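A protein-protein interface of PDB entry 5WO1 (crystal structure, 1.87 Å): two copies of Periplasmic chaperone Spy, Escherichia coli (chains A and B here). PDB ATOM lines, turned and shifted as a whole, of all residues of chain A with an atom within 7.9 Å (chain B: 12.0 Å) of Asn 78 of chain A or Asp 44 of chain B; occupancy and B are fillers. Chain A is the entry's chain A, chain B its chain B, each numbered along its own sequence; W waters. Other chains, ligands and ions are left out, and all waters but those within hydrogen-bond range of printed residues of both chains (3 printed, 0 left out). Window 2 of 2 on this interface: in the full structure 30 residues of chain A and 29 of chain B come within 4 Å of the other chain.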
ATOM      1  N   PHE A   2      -7.849 -11.394 -37.605  1.00  0.00           N
ATOM      2  CA  PHE A   2      -8.015 -12.816 -37.296  1.00  0.00           C
ATOM      3  C   PHE A   2      -7.511 -13.735 -38.401  1.00  0.00           C
ATOM      4  O   PHE A   2      -7.063 -14.850 -38.113  1.00  0.00           O
ATOM      5  CB  PHE A   2      -9.482 -13.125 -37.007  1.00  0.00           C
ATOM      6  CG  PHE A   2      -9.971 -12.534 -35.726  1.00  0.00           C
ATOM      7  CD1 PHE A   2     -10.541 -11.286 -35.711  1.00  0.00           C
ATOM      8  CD2 PHE A   2      -9.835 -13.219 -34.535  1.00  0.00           C
ATOM      9  CE1 PHE A   2     -10.981 -10.737 -34.539  1.00  0.00           C
ATOM     10  CE2 PHE A   2     -10.275 -12.669 -33.343  1.00  0.00           C
ATOM     11  CZ  PHE A   2     -10.854 -11.432 -33.344  1.00  0.00           C
ATOM     12  N   GLN A  11     -10.847 -24.140 -36.555  1.00  0.00           N
ATOM     13  CA  GLN A  11     -11.140 -22.750 -36.188  1.00  0.00           C
ATOM     14  C   GLN A  11     -11.954 -22.045 -37.265  1.00  0.00           C
ATOM     15  O   GLN A  11     -12.856 -21.262 -36.953  1.00  0.00           O
ATOM     16  CB  GLN A  11      -9.846 -21.995 -35.905  1.00  0.00           C
ATOM     17  CG  GLN A  11      -9.189 -22.438 -34.598  1.00  0.00           C
ATOM     18  CD  GLN A  11      -7.809 -21.809 -34.397  1.00  0.00           C
ATOM     19  OE1 GLN A  11      -7.097 -21.547 -35.365  1.00  0.00           O
ATOM     20  NE2 GLN A  11      -7.443 -21.535 -33.144  1.00  0.00           N
ATOM     21  N   GLN A  14     -15.479 -23.097 -36.699  1.00  0.00           N
ATOM     22  CA  GLN A  14     -15.999 -22.461 -35.491  1.00  0.00           C
ATOM     23  C   GLN A  14     -16.328 -20.994 -35.725  1.00  0.00           C
ATOM     24  O   GLN A  14     -17.340 -20.486 -35.229  1.00  0.00           O
ATOM     25  CB  GLN A  14     -14.982 -22.607 -34.367  1.00  0.00           C
ATOM     26  CG  GLN A  14     -14.760 -24.077 -33.944  1.00  0.00           C
ATOM     27  CD  GLN A  14     -13.661 -24.226 -32.929  1.00  0.00           C
ATOM     28  OE1 GLN A  14     -12.508 -23.899 -33.204  1.00  0.00           O
ATOM     29  NE2 GLN A  14     -14.009 -24.689 -31.737  1.00  0.00           N
ATOM     30  N   ILE A  18     -19.853 -19.058 -35.344  1.00  0.00           N
ATOM     31  CA  ILE A  18     -20.001 -17.887 -34.484  1.00  0.00           C
ATOM     32  C   ILE A  18     -20.665 -16.744 -35.242  1.00  0.00           C
ATOM     33  O   ILE A  18     -21.480 -16.002 -34.682  1.00  0.00           O
ATOM     34  CB  ILE A  18     -18.632 -17.467 -33.910  1.00  0.00           C
ATOM     35  CG1 ILE A  18     -18.142 -18.520 -32.904  1.00  0.00           C
ATOM     36  CG2 ILE A  18     -18.755 -16.092 -33.255  1.00  0.00           C
ATOM     37  CD1 ILE A  18     -16.642 -18.385 -32.503  1.00  0.00           C
ATOM     38  N   GLU A  71     -19.254  -9.329 -28.590  1.00  0.00           N
ATOM     39  CA  GLU A  71     -19.454 -10.714 -28.155  1.00  0.00           C
ATOM     40  C   GLU A  71     -18.865 -11.685 -29.153  1.00  0.00           C
ATOM     41  O   GLU A  71     -18.270 -12.705 -28.759  1.00  0.00           O
ATOM     42  CB  GLU A  71     -20.924 -11.025 -27.954  1.00  0.00           C
ATOM     43  CG  GLU A  71     -21.084 -12.430 -27.368  1.00  0.00           C
ATOM     44  CD  GLU A  71     -22.481 -12.750 -26.836  1.00  0.00           C
ATOM     45  OE1 GLU A  71     -23.431 -12.014 -27.106  1.00  0.00           O
ATOM     46  OE2 GLU A  71     -22.633 -13.786 -26.161  1.00  0.00           O
ATOM     47  N   THR A  72     -19.070 -11.399 -30.443  1.00  0.00           N
ATOM     48  CA  THR A  72     -18.469 -12.189 -31.514  1.00  0.00           C
ATOM     49  C   THR A  72     -16.952 -12.180 -31.401  1.00  0.00           C
ATOM     50  O   THR A  72     -16.311 -13.230 -31.486  1.00  0.00           O
ATOM     51  CB  THR A  72     -18.931 -11.636 -32.862  1.00  0.00           C
ATOM     52  OG1 THR A  72     -20.342 -11.869 -33.008  1.00  0.00           O
ATOM     53  CG2 THR A  72     -18.207 -12.330 -34.019  1.00  0.00           C
ATOM     54  N   GLN A  73     -16.365 -10.998 -31.227  1.00  0.00           N
ATOM     55  CA  GLN A  73     -14.921 -10.901 -31.043  1.00  0.00           C
ATOM     56  C   GLN A  73     -14.469 -11.743 -29.863  1.00  0.00           C
ATOM     57  O   GLN A  73     -13.498 -12.482 -29.974  1.00  0.00           O
ATOM     58  CB  GLN A  73     -14.485  -9.453 -30.857  1.00  0.00           C
ATOM     59  CG  GLN A  73     -14.440  -8.615 -32.152  1.00  0.00           C
ATOM     60  CD  GLN A  73     -14.189  -7.125 -31.892  1.00  0.00           C
ATOM     61  OE1 GLN A  73     -14.636  -6.576 -30.888  1.00  0.00           O
ATOM     62  NE2 GLN A  73     -13.466  -6.478 -32.792  1.00  0.00           N
ATOM     63  N   ASN A  74     -15.147 -11.614 -28.711  1.00  0.00           N
ATOM     64  CA  ASN A  74     -14.759 -12.371 -27.528  1.00  0.00           C
ATOM     65  C   ASN A  74     -14.827 -13.859 -27.810  1.00  0.00           C
ATOM     66  O   ASN A  74     -13.957 -14.620 -27.376  1.00  0.00           O
ATOM     67  CB  ASN A  74     -15.664 -11.996 -26.334  1.00  0.00           C
ATOM     68  CG  ASN A  74     -15.367 -12.811 -25.099  1.00  0.00           C
ATOM     69  OD1 ASN A  74     -15.964 -13.840 -24.864  1.00  0.00           O
ATOM     70  ND2 ASN A  74     -14.424 -12.364 -24.321  1.00  0.00           N
ATOM     71  N   LYS A  75     -15.879 -14.301 -28.490  1.00  0.00           N
ATOM     72  CA  LYS A  75     -16.012 -15.729 -28.811  1.00  0.00           C
ATOM     73  C   LYS A  75     -14.861 -16.211 -29.701  1.00  0.00           C
ATOM     74  O   LYS A  75     -14.285 -17.291 -29.488  1.00  0.00           O
ATOM     75  CB  LYS A  75     -17.341 -15.964 -29.508  1.00  0.00           C
ATOM     76  CG  LYS A  75     -18.498 -16.151 -28.532  1.00  0.00           C
ATOM     77  CD  LYS A  75     -19.797 -16.073 -29.280  1.00  0.00           C
ATOM     78  CE  LYS A  75     -20.958 -16.494 -28.395  1.00  0.00           C
ATOM     79  NZ  LYS A  75     -22.203 -16.431 -29.169  1.00  0.00           N
ATOM     80  N   ILE A  76     -14.499 -15.421 -30.693  1.00  0.00           N
ATOM     81  CA  ILE A  76     -13.419 -15.856 -31.576  1.00  0.00           C
ATOM     82  C   ILE A  76     -12.095 -15.854 -30.811  1.00  0.00           C
ATOM     83  O   ILE A  76     -11.274 -16.776 -30.950  1.00  0.00           O
ATOM     84  CB  ILE A  76     -13.353 -14.988 -32.828  1.00  0.00           C
ATOM     85  CG1 ILE A  76     -14.658 -15.093 -33.639  1.00  0.00           C
ATOM     86  CG2 ILE A  76     -12.167 -15.465 -33.693  1.00  0.00           C
ATOM     87  CD1 ILE A  76     -14.764 -14.077 -34.781  1.00  0.00           C
ATOM     88  N   TYR A  77     -11.871 -14.823 -29.987  1.00  0.00           N
ATOM     89  CA  TYR A  77     -10.614 -14.742 -29.241  1.00  0.00           C
ATOM     90  C   TYR A  77     -10.434 -16.018 -28.449  1.00  0.00           C
ATOM     91  O   TYR A  77      -9.342 -16.588 -28.379  1.00  0.00           O
ATOM     92  CB  TYR A  77     -10.633 -13.554 -28.286  1.00  0.00           C
ATOM     93  CG  TYR A  77      -9.392 -13.466 -27.413  1.00  0.00           C
ATOM     94  CD1 TYR A  77      -8.286 -12.738 -27.830  1.00  0.00           C
ATOM     95  CD2 TYR A  77      -9.343 -14.072 -26.149  1.00  0.00           C
ATOM     96  CE1 TYR A  77      -7.156 -12.616 -27.029  1.00  0.00           C
ATOM     97  CE2 TYR A  77      -8.196 -13.941 -25.326  1.00  0.00           C
ATOM     98  CZ  TYR A  77      -7.111 -13.235 -25.773  1.00  0.00           C
ATOM     99  OH  TYR A  77      -5.959 -13.124 -24.987  1.00  0.00           O
ATOM    100  N   ASN A  78     -11.517 -16.502 -27.876  1.00  0.00           N
ATOM    101  CA  ASN A  78     -11.380 -17.659 -27.009  1.00  0.00           C
ATOM    102  C   ASN A  78     -11.179 -18.984 -27.739  1.00  0.00           C
ATOM    103  O   ASN A  78     -10.783 -19.927 -27.081  1.00  0.00           O
ATOM    104  CB  ASN A  78     -12.560 -17.747 -26.081  1.00  0.00           C
ATOM    105  CG  ASN A  78     -12.338 -16.924 -24.844  1.00  0.00           C
ATOM    106  OD1 ASN A  78     -11.533 -17.298 -23.966  1.00  0.00           O
ATOM    107  ND2 ASN A  78     -12.983 -15.751 -24.787  1.00  0.00           N
ATOM    108  N   ILE A  79     -11.367 -19.089 -29.058  1.00  0.00           N
ATOM    109  CA  ILE A  79     -10.995 -20.343 -29.730  1.00  0.00           C
ATOM    110  C   ILE A  79      -9.546 -20.344 -30.153  1.00  0.00           C
ATOM    111  O   ILE A  79      -9.071 -21.376 -30.660  1.00  0.00           O
ATOM    112  CB  ILE A  79     -11.812 -20.670 -31.000  1.00  0.00           C
ATOM    113  CG1 ILE A  79     -11.496 -19.690 -32.141  1.00  0.00           C
ATOM    114  CG2 ILE A  79     -13.299 -20.647 -30.669  1.00  0.00           C
ATOM    115  CD1 ILE A  79     -12.226 -19.959 -33.408  1.00  0.00           C
ATOM    116  N   LEU A  80      -8.833 -19.230 -29.982  1.00  0.00           N
ATOM    117  CA  LEU A  80      -7.414 -19.148 -30.314  1.00  0.00           C
ATOM    118  C   LEU A  80      -6.544 -19.946 -29.367  1.00  0.00           C
ATOM    119  O   LEU A  80      -6.869 -20.136 -28.196  1.00  0.00           O
ATOM    120  CB  LEU A  80      -6.935 -17.691 -30.299  1.00  0.00           C
ATOM    121  CG  LEU A  80      -7.725 -16.869 -31.292  1.00  0.00           C
ATOM    122  CD1 LEU A  80      -7.213 -15.409 -31.193  1.00  0.00           C
ATOM    123  CD2 LEU A  80      -7.683 -17.443 -32.727  1.00  0.00           C
ATOM    124  N   THR A  81      -5.385 -20.377 -29.886  1.00  0.00           N
ATOM    125  CA  THR A  81      -4.374 -20.961 -29.055  1.00  0.00           C
ATOM    126  C   THR A  81      -3.601 -19.884 -28.287  1.00  0.00           C
ATOM    127  O   THR A  81      -3.614 -18.704 -28.644  1.00  0.00           O
ATOM    128  CB  THR A  81      -3.359 -21.753 -29.892  1.00  0.00           C
ATOM    129  OG1 THR A  81      -2.677 -20.829 -30.750  1.00  0.00           O
ATOM    130  CG2 THR A  81      -4.010 -22.847 -30.703  1.00  0.00           C
ATOM    131  N   LYS A  85      -3.343 -16.027 -29.479  1.00  0.00           N
ATOM    132  CA  LYS A  85      -3.782 -14.916 -28.635  1.00  0.00           C
ATOM    133  C   LYS A  85      -2.675 -13.876 -28.461  1.00  0.00           C
ATOM    134  O   LYS A  85      -2.949 -12.672 -28.453  1.00  0.00           O
ATOM    135  CB  LYS A  85      -4.227 -15.441 -27.272  1.00  0.00           C
ATOM    136  CG  LYS A  85      -5.471 -16.246 -27.287  1.00  0.00           C
ATOM    137  CD  LYS A  85      -5.780 -16.750 -25.869  1.00  0.00           C
ATOM    138  CE  LYS A  85      -7.169 -17.369 -25.763  1.00  0.00           C
ATOM    139  NZ  LYS A  85      -7.266 -18.197 -24.582  1.00  0.00           N
ATOM    140  N   ALA B  36     -10.026  -0.599 -22.290  1.00  0.00           N
ATOM    141  CA  ALA B  36     -11.174  -1.290 -21.724  1.00  0.00           C
ATOM    142  C   ALA B  36     -11.823  -2.214 -22.755  1.00  0.00           C
ATOM    143  O   ALA B  36     -12.230  -3.336 -22.430  1.00  0.00           O
ATOM    144  CB  ALA B  36     -12.181  -0.257 -21.188  1.00  0.00           C
ATOM    145  N   MET B  37     -11.922  -1.776 -24.003  1.00  0.00           N
ATOM    146  CA  MET B  37     -12.399  -2.683 -25.050  1.00  0.00           C
ATOM    147  C   MET B  37     -11.512  -3.911 -25.173  1.00  0.00           C
ATOM    148  O   MET B  37     -11.995  -5.039 -25.342  1.00  0.00           O
ATOM    149  CB  MET B  37     -12.428  -1.944 -26.376  1.00  0.00           C
ATOM    150  CG  MET B  37     -12.689  -2.801 -27.578  1.00  0.00           C
ATOM    151  SD  MET B  37     -14.411  -3.225 -27.633  1.00  0.00           S
ATOM    152  CE  MET B  37     -14.969  -2.025 -28.821  1.00  0.00           C
ATOM    153  N   HIS B  38     -10.201  -3.711 -25.168  1.00  0.00           N
ATOM    154  CA  HIS B  38      -9.305  -4.861 -25.250  1.00  0.00           C
ATOM    155  C   HIS B  38      -9.632  -5.875 -24.172  1.00  0.00           C
ATOM    156  O   HIS B  38      -9.715  -7.081 -24.431  1.00  0.00           O
ATOM    157  CB  HIS B  38      -7.872  -4.397 -25.112  1.00  0.00           C
ATOM    158  CG  HIS B  38      -6.869  -5.419 -25.552  1.00  0.00           C
ATOM    159  ND1 HIS B  38      -5.522  -5.200 -25.474  1.00  0.00           N
ATOM    160  CD2 HIS B  38      -7.009  -6.679 -26.043  1.00  0.00           C
ATOM    161  CE1 HIS B  38      -4.859  -6.248 -25.923  1.00  0.00           C
ATOM    162  NE2 HIS B  38      -5.743  -7.170 -26.261  1.00  0.00           N
ATOM    163  N   ASP B  39      -9.842  -5.386 -22.949  1.00  0.00           N
ATOM    164  CA  ASP B  39     -10.070  -6.252 -21.799  1.00  0.00           C
ATOM    165  C   ASP B  39     -11.398  -6.984 -21.901  1.00  0.00           C
ATOM    166  O   ASP B  39     -11.505  -8.116 -21.431  1.00  0.00           O
ATOM    167  CB  ASP B  39     -10.005  -5.415 -20.530  1.00  0.00           C
ATOM    168  CG  ASP B  39      -8.597  -4.939 -20.253  1.00  0.00           C
ATOM    169  OD1 ASP B  39      -7.657  -5.486 -20.912  1.00  0.00           O
ATOM    170  OD2 ASP B  39      -8.451  -4.022 -19.435  1.00  0.00           O
ATOM    171  N   ILE B  40     -12.382  -6.388 -22.561  1.00  0.00           N
ATOM    172  CA  ILE B  40     -13.640  -7.092 -22.765  1.00  0.00           C
ATOM    173  C   ILE B  40     -13.464  -8.218 -23.775  1.00  0.00           C
ATOM    174  O   ILE B  40     -14.009  -9.319 -23.607  1.00  0.00           O
ATOM    175  CB  ILE B  40     -14.728  -6.110 -23.220  1.00  0.00           C
ATOM    176  CG1 ILE B  40     -15.083  -5.200 -22.044  1.00  0.00           C
ATOM    177  CG2 ILE B  40     -15.994  -6.850 -23.601  1.00  0.00           C
ATOM    178  CD1 ILE B  40     -15.842  -4.023 -22.399  1.00  0.00           C
ATOM    179  N   ILE B  41     -12.719  -7.952 -24.847  1.00  0.00           N
ATOM    180  CA  ILE B  41     -12.517  -8.953 -25.885  1.00  0.00           C
ATOM    181  C   ILE B  41     -11.642 -10.094 -25.365  1.00  0.00           C
ATOM    182  O   ILE B  41     -11.895 -11.274 -25.649  1.00  0.00           O
ATOM    183  CB  ILE B  41     -11.903  -8.307 -27.135  1.00  0.00           C
ATOM    184  CG1 ILE B  41     -12.865  -7.329 -27.811  1.00  0.00           C
ATOM    185  CG2 ILE B  41     -11.377  -9.417 -28.126  1.00  0.00           C
ATOM    186  CD1 ILE B  41     -12.232  -6.650 -28.971  1.00  0.00           C
ATOM    187  N   ALA B  42     -10.601  -9.774 -24.611  1.00  0.00           N
ATOM    188  CA  ALA B  42      -9.645 -10.792 -24.198  1.00  0.00           C
ATOM    189  C   ALA B  42     -10.083 -11.576 -22.957  1.00  0.00           C
ATOM    190  O   ALA B  42      -9.345 -12.448 -22.498  1.00  0.00           O
ATOM    191  CB  ALA B  42      -8.276 -10.184 -23.933  1.00  0.00           C
ATOM    192  N   SER B  43     -11.282 -11.368 -22.469  1.00  0.00           N
ATOM    193  CA  SER B  43     -11.723 -12.002 -21.239  1.00  0.00           C
ATOM    194  C   SER B  43     -12.141 -13.455 -21.494  1.00  0.00           C
ATOM    195  O   SER B  43     -12.589 -13.798 -22.583  1.00  0.00           O
ATOM    196  CB  SER B  43     -12.877 -11.179 -20.676  1.00  0.00           C
ATOM    197  OG  SER B  43     -13.317 -11.754 -19.492  1.00  0.00           O
ATOM    198  N   ASP B  44     -12.022 -14.306 -20.451  1.00  0.00           N
ATOM    199  CA  ASP B  44     -12.409 -15.710 -20.590  1.00  0.00           C
ATOM    200  C   ASP B  44     -13.913 -15.838 -20.874  1.00  0.00           C
ATOM    201  O   ASP B  44     -14.350 -16.786 -21.514  1.00  0.00           O
ATOM    202  CB  ASP B  44     -12.045 -16.498 -19.319  1.00  0.00           C
ATOM    203  CG  ASP B  44     -10.587 -16.935 -19.263  1.00  0.00           C
ATOM    204  OD1 ASP B  44      -9.786 -16.555 -20.134  1.00  0.00           O
ATOM    205  OD2 ASP B  44     -10.198 -17.689 -18.325  1.00  0.00           O
ATOM    206  N   THR B  45     -14.729 -14.905 -20.375  1.00  0.00           N
ATOM    207  CA  THR B  45     -16.164 -14.908 -20.655  1.00  0.00           C
ATOM    208  C   THR B  45     -16.605 -13.516 -21.104  1.00  0.00           C
ATOM    209  O   THR B  45     -15.958 -12.526 -20.784  1.00  0.00           O
ATOM    210  CB  THR B  45     -16.972 -15.268 -19.416  1.00  0.00           C
ATOM    211  OG1 THR B  45     -16.524 -14.438 -18.338  1.00  0.00           O
ATOM    212  CG2 THR B  45     -16.808 -16.748 -19.057  1.00  0.00           C
ATOM    213  N   PHE B  46     -17.747 -13.434 -21.799  1.00  0.00           N
ATOM    214  CA  PHE B  46     -18.291 -12.141 -22.202  1.00  0.00           C
ATOM    215  C   PHE B  46     -19.200 -11.593 -21.096  1.00  0.00           C
ATOM    216  O   PHE B  46     -20.144 -12.250 -20.647  1.00  0.00           O
ATOM    217  CB  PHE B  46     -19.041 -12.269 -23.534  1.00  0.00           C
ATOM    218  CG  PHE B  46     -19.627 -10.970 -24.021  1.00  0.00           C
ATOM    219  CD1 PHE B  46     -18.798  -9.978 -24.456  1.00  0.00           C
ATOM    220  CD2 PHE B  46     -20.995 -10.772 -24.055  1.00  0.00           C
ATOM    221  CE1 PHE B  46     -19.300  -8.772 -24.910  1.00  0.00           C
ATOM    222  CE2 PHE B  46     -21.518  -9.564 -24.501  1.00  0.00           C
ATOM    223  CZ  PHE B  46     -20.651  -8.566 -24.941  1.00  0.00           C
ATOM    224  N   ASP B  47     -18.927 -10.386 -20.660  1.00  0.00           N
ATOM    225  CA  ASP B  47     -19.661  -9.797 -19.569  1.00  0.00           C
ATOM    226  C   ASP B  47     -20.532  -8.710 -20.170  1.00  0.00           C
ATOM    227  O   ASP B  47     -20.022  -7.646 -20.473  1.00  0.00           O
ATOM    228  CB  ASP B  47     -18.685  -9.230 -18.577  1.00  0.00           C
ATOM    229  CG  ASP B  47     -19.348  -8.646 -17.369  1.00  0.00           C
ATOM    230  OD1 ASP B  47     -20.504  -8.112 -17.406  1.00  0.00           O
ATOM    231  OD2 ASP B  47     -18.628  -8.713 -16.355  1.00  0.00           O
ATOM    232  N   LYS B  48     -21.826  -8.976 -20.348  1.00  0.00           N
ATOM    233  CA  LYS B  48     -22.661  -8.048 -21.120  1.00  0.00           C
ATOM    234  C   LYS B  48     -22.823  -6.733 -20.398  1.00  0.00           C
ATOM    235  O   LYS B  48     -22.767  -5.656 -21.026  1.00  0.00           O
ATOM    236  CB  LYS B  48     -24.028  -8.672 -21.412  1.00  0.00           C
ATOM    237  CG  LYS B  48     -24.943  -7.768 -22.223  1.00  0.00           C
ATOM    238  CD  LYS B  48     -26.181  -8.453 -22.855  1.00  0.00           C
ATOM    239  CE  LYS B  48     -25.848  -9.601 -23.835  1.00  0.00           C
ATOM    240  NZ  LYS B  48     -25.690  -9.225 -25.283  1.00  0.00           N
ATOM    241  N   LYS B  50     -20.780  -5.225 -18.275  1.00  0.00           N
ATOM    242  CA  LYS B  50     -19.549  -4.457 -18.443  1.00  0.00           C
ATOM    243  C   LYS B  50     -19.418  -3.926 -19.866  1.00  0.00           C
ATOM    244  O   LYS B  50     -18.954  -2.800 -20.077  1.00  0.00           O
ATOM    245  CB  LYS B  50     -18.364  -5.365 -18.105  1.00  0.00           C
ATOM    246  CG  LYS B  50     -17.065  -4.648 -17.848  1.00  0.00           C
ATOM    247  CD  LYS B  50     -15.980  -5.634 -17.355  1.00  0.00           C
ATOM    248  CE  LYS B  50     -16.380  -6.350 -16.055  1.00  0.00           C
ATOM    249  NZ  LYS B  50     -16.852  -5.395 -15.005  1.00  0.00           N
HETATM  250  O   HOH W   1     -23.980  -9.561 -27.212  1.00  0.00           O
HETATM  251  O   HOH W   2     -16.022 -16.261 -24.068  1.00  0.00           O
HETATM  252  O   HOH W   3      -9.420 -16.095 -22.711  1.00  0.00           O
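The side-chain amide nitrogen (ND2) of Asn 74 of chain A is in hydrogen-bond range of the backbone carbonyl oxygen (O) of Ile 40 of chain B, 3.2 Å away.
The side-chain amide nitrogen of Asn 74 of chain A is in hydrogen-bond range of the backbone carbonyl oxygen of Ile 41 of chain B, 3.1 Å away.
The side-chain amide nitrogen of Asn 74 of chain A is in hydrogen-bond range of the backbone carbonyl oxygen of Ser 43 of chain B (2.9 Å).
ND2 of Asn 78 of chain A is in hydrogen-bond range of O of Ser 43 of chain B.
The side-chain hydroxyl (OG) of Ser 43 of chain B lies within hydrogen-bond range of the backbone carbonyl oxygen (O) of Thr 45 of chain B (3.0 Å).
O of Asn 74 of chain A lies within hydrogen-bond range of ND2 of Asn 78 of chain A (3.0 Å).
Phe 46 of chain B touches Glu 71 of chain A.
Gln 73 of chain A touches Ile 41 of chain B.
Thr 45 of chain B touches Asn 74 of chain A (C to OD1, 3.8 Å).
Asn 74 of chain A touches Phe 46 of chain B (OD1 to N, 3.6 Å).
Tyr 77 of chain A touches Ile 41 of chain B.
Ala 42 of chain B touches Tyr 77 of chain A.
Asn 78 of chain A touches Asp 44 of chain B (ND2 to O, 3.7 Å).
Asn 78 of chain A touches just these residues of chain B: Ser 43 (3.0 Å) and Asp 44 (3.7 Å).
Of the printed residues of chain B, Asn 74 of chain A touches Ile 40, Ile 41, Ser 43, Thr 45 and Phe 46.
Tyr 77 of chain A touches just these residues of chain B: Ile 41 (3.7 Å) and Ala 42 (3.4 Å).
No residue of chain B comes within 4 Å of Ile 79 of chain A.
Of chain A, only Asn 74 (2.9 Å) and Asn 78 (3.0 Å) come within 4 Å of Ser 43 of chain B.
Printed residues of chain A within 4 Å of Ile 40 of chain B: Asn 74 (3.2 Å).
Printed residues of chain A within 4 Å of Ala 42 of chain B: Tyr 77 (3.4 Å).
Printed residues of chain B within 4 Å of Glu 71 of chain A: Phe 46.
Ala 36 of chain B touches none of the printed residues of chain A.
The nearest residue of chain A that does not touch Asp 44 of chain B is Asn 74 of chain A (4.7 Å).
Hydrophobic or aromatic side chains of chain A within 4 Å of the printed part of chain B: Tyr 77.
Among the printed residues, 11 pairs touch across the chains.
Among the printed residues, no Asp or Glu carboxylate lies within 4 Å of a Lys or Arg side-chain nitrogen of the other chain.
No position is printed for both chains.
Of the 11 pairs that touch across the chains among the printed residues, none has its exchanged pair printed and touching as well.
Water W1 bridges the side-chain carboxylate of Glu 71 of chain A (2.5 Å) and the side-chain amino group of Lys 48 of chain B (2.6 Å).
Water W2 lies within hydrogen-bond range of OD1 of Asn 74 of chain A, O of Asp 44 of chain B and ND2 of Asn 78 of chain A.
Water W3 bridges the side-chain carboxylate of Asp 44 of chain B (2.6 Å) and the side-chain amide oxygen of Asn 78 of chain A (2.7 Å).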
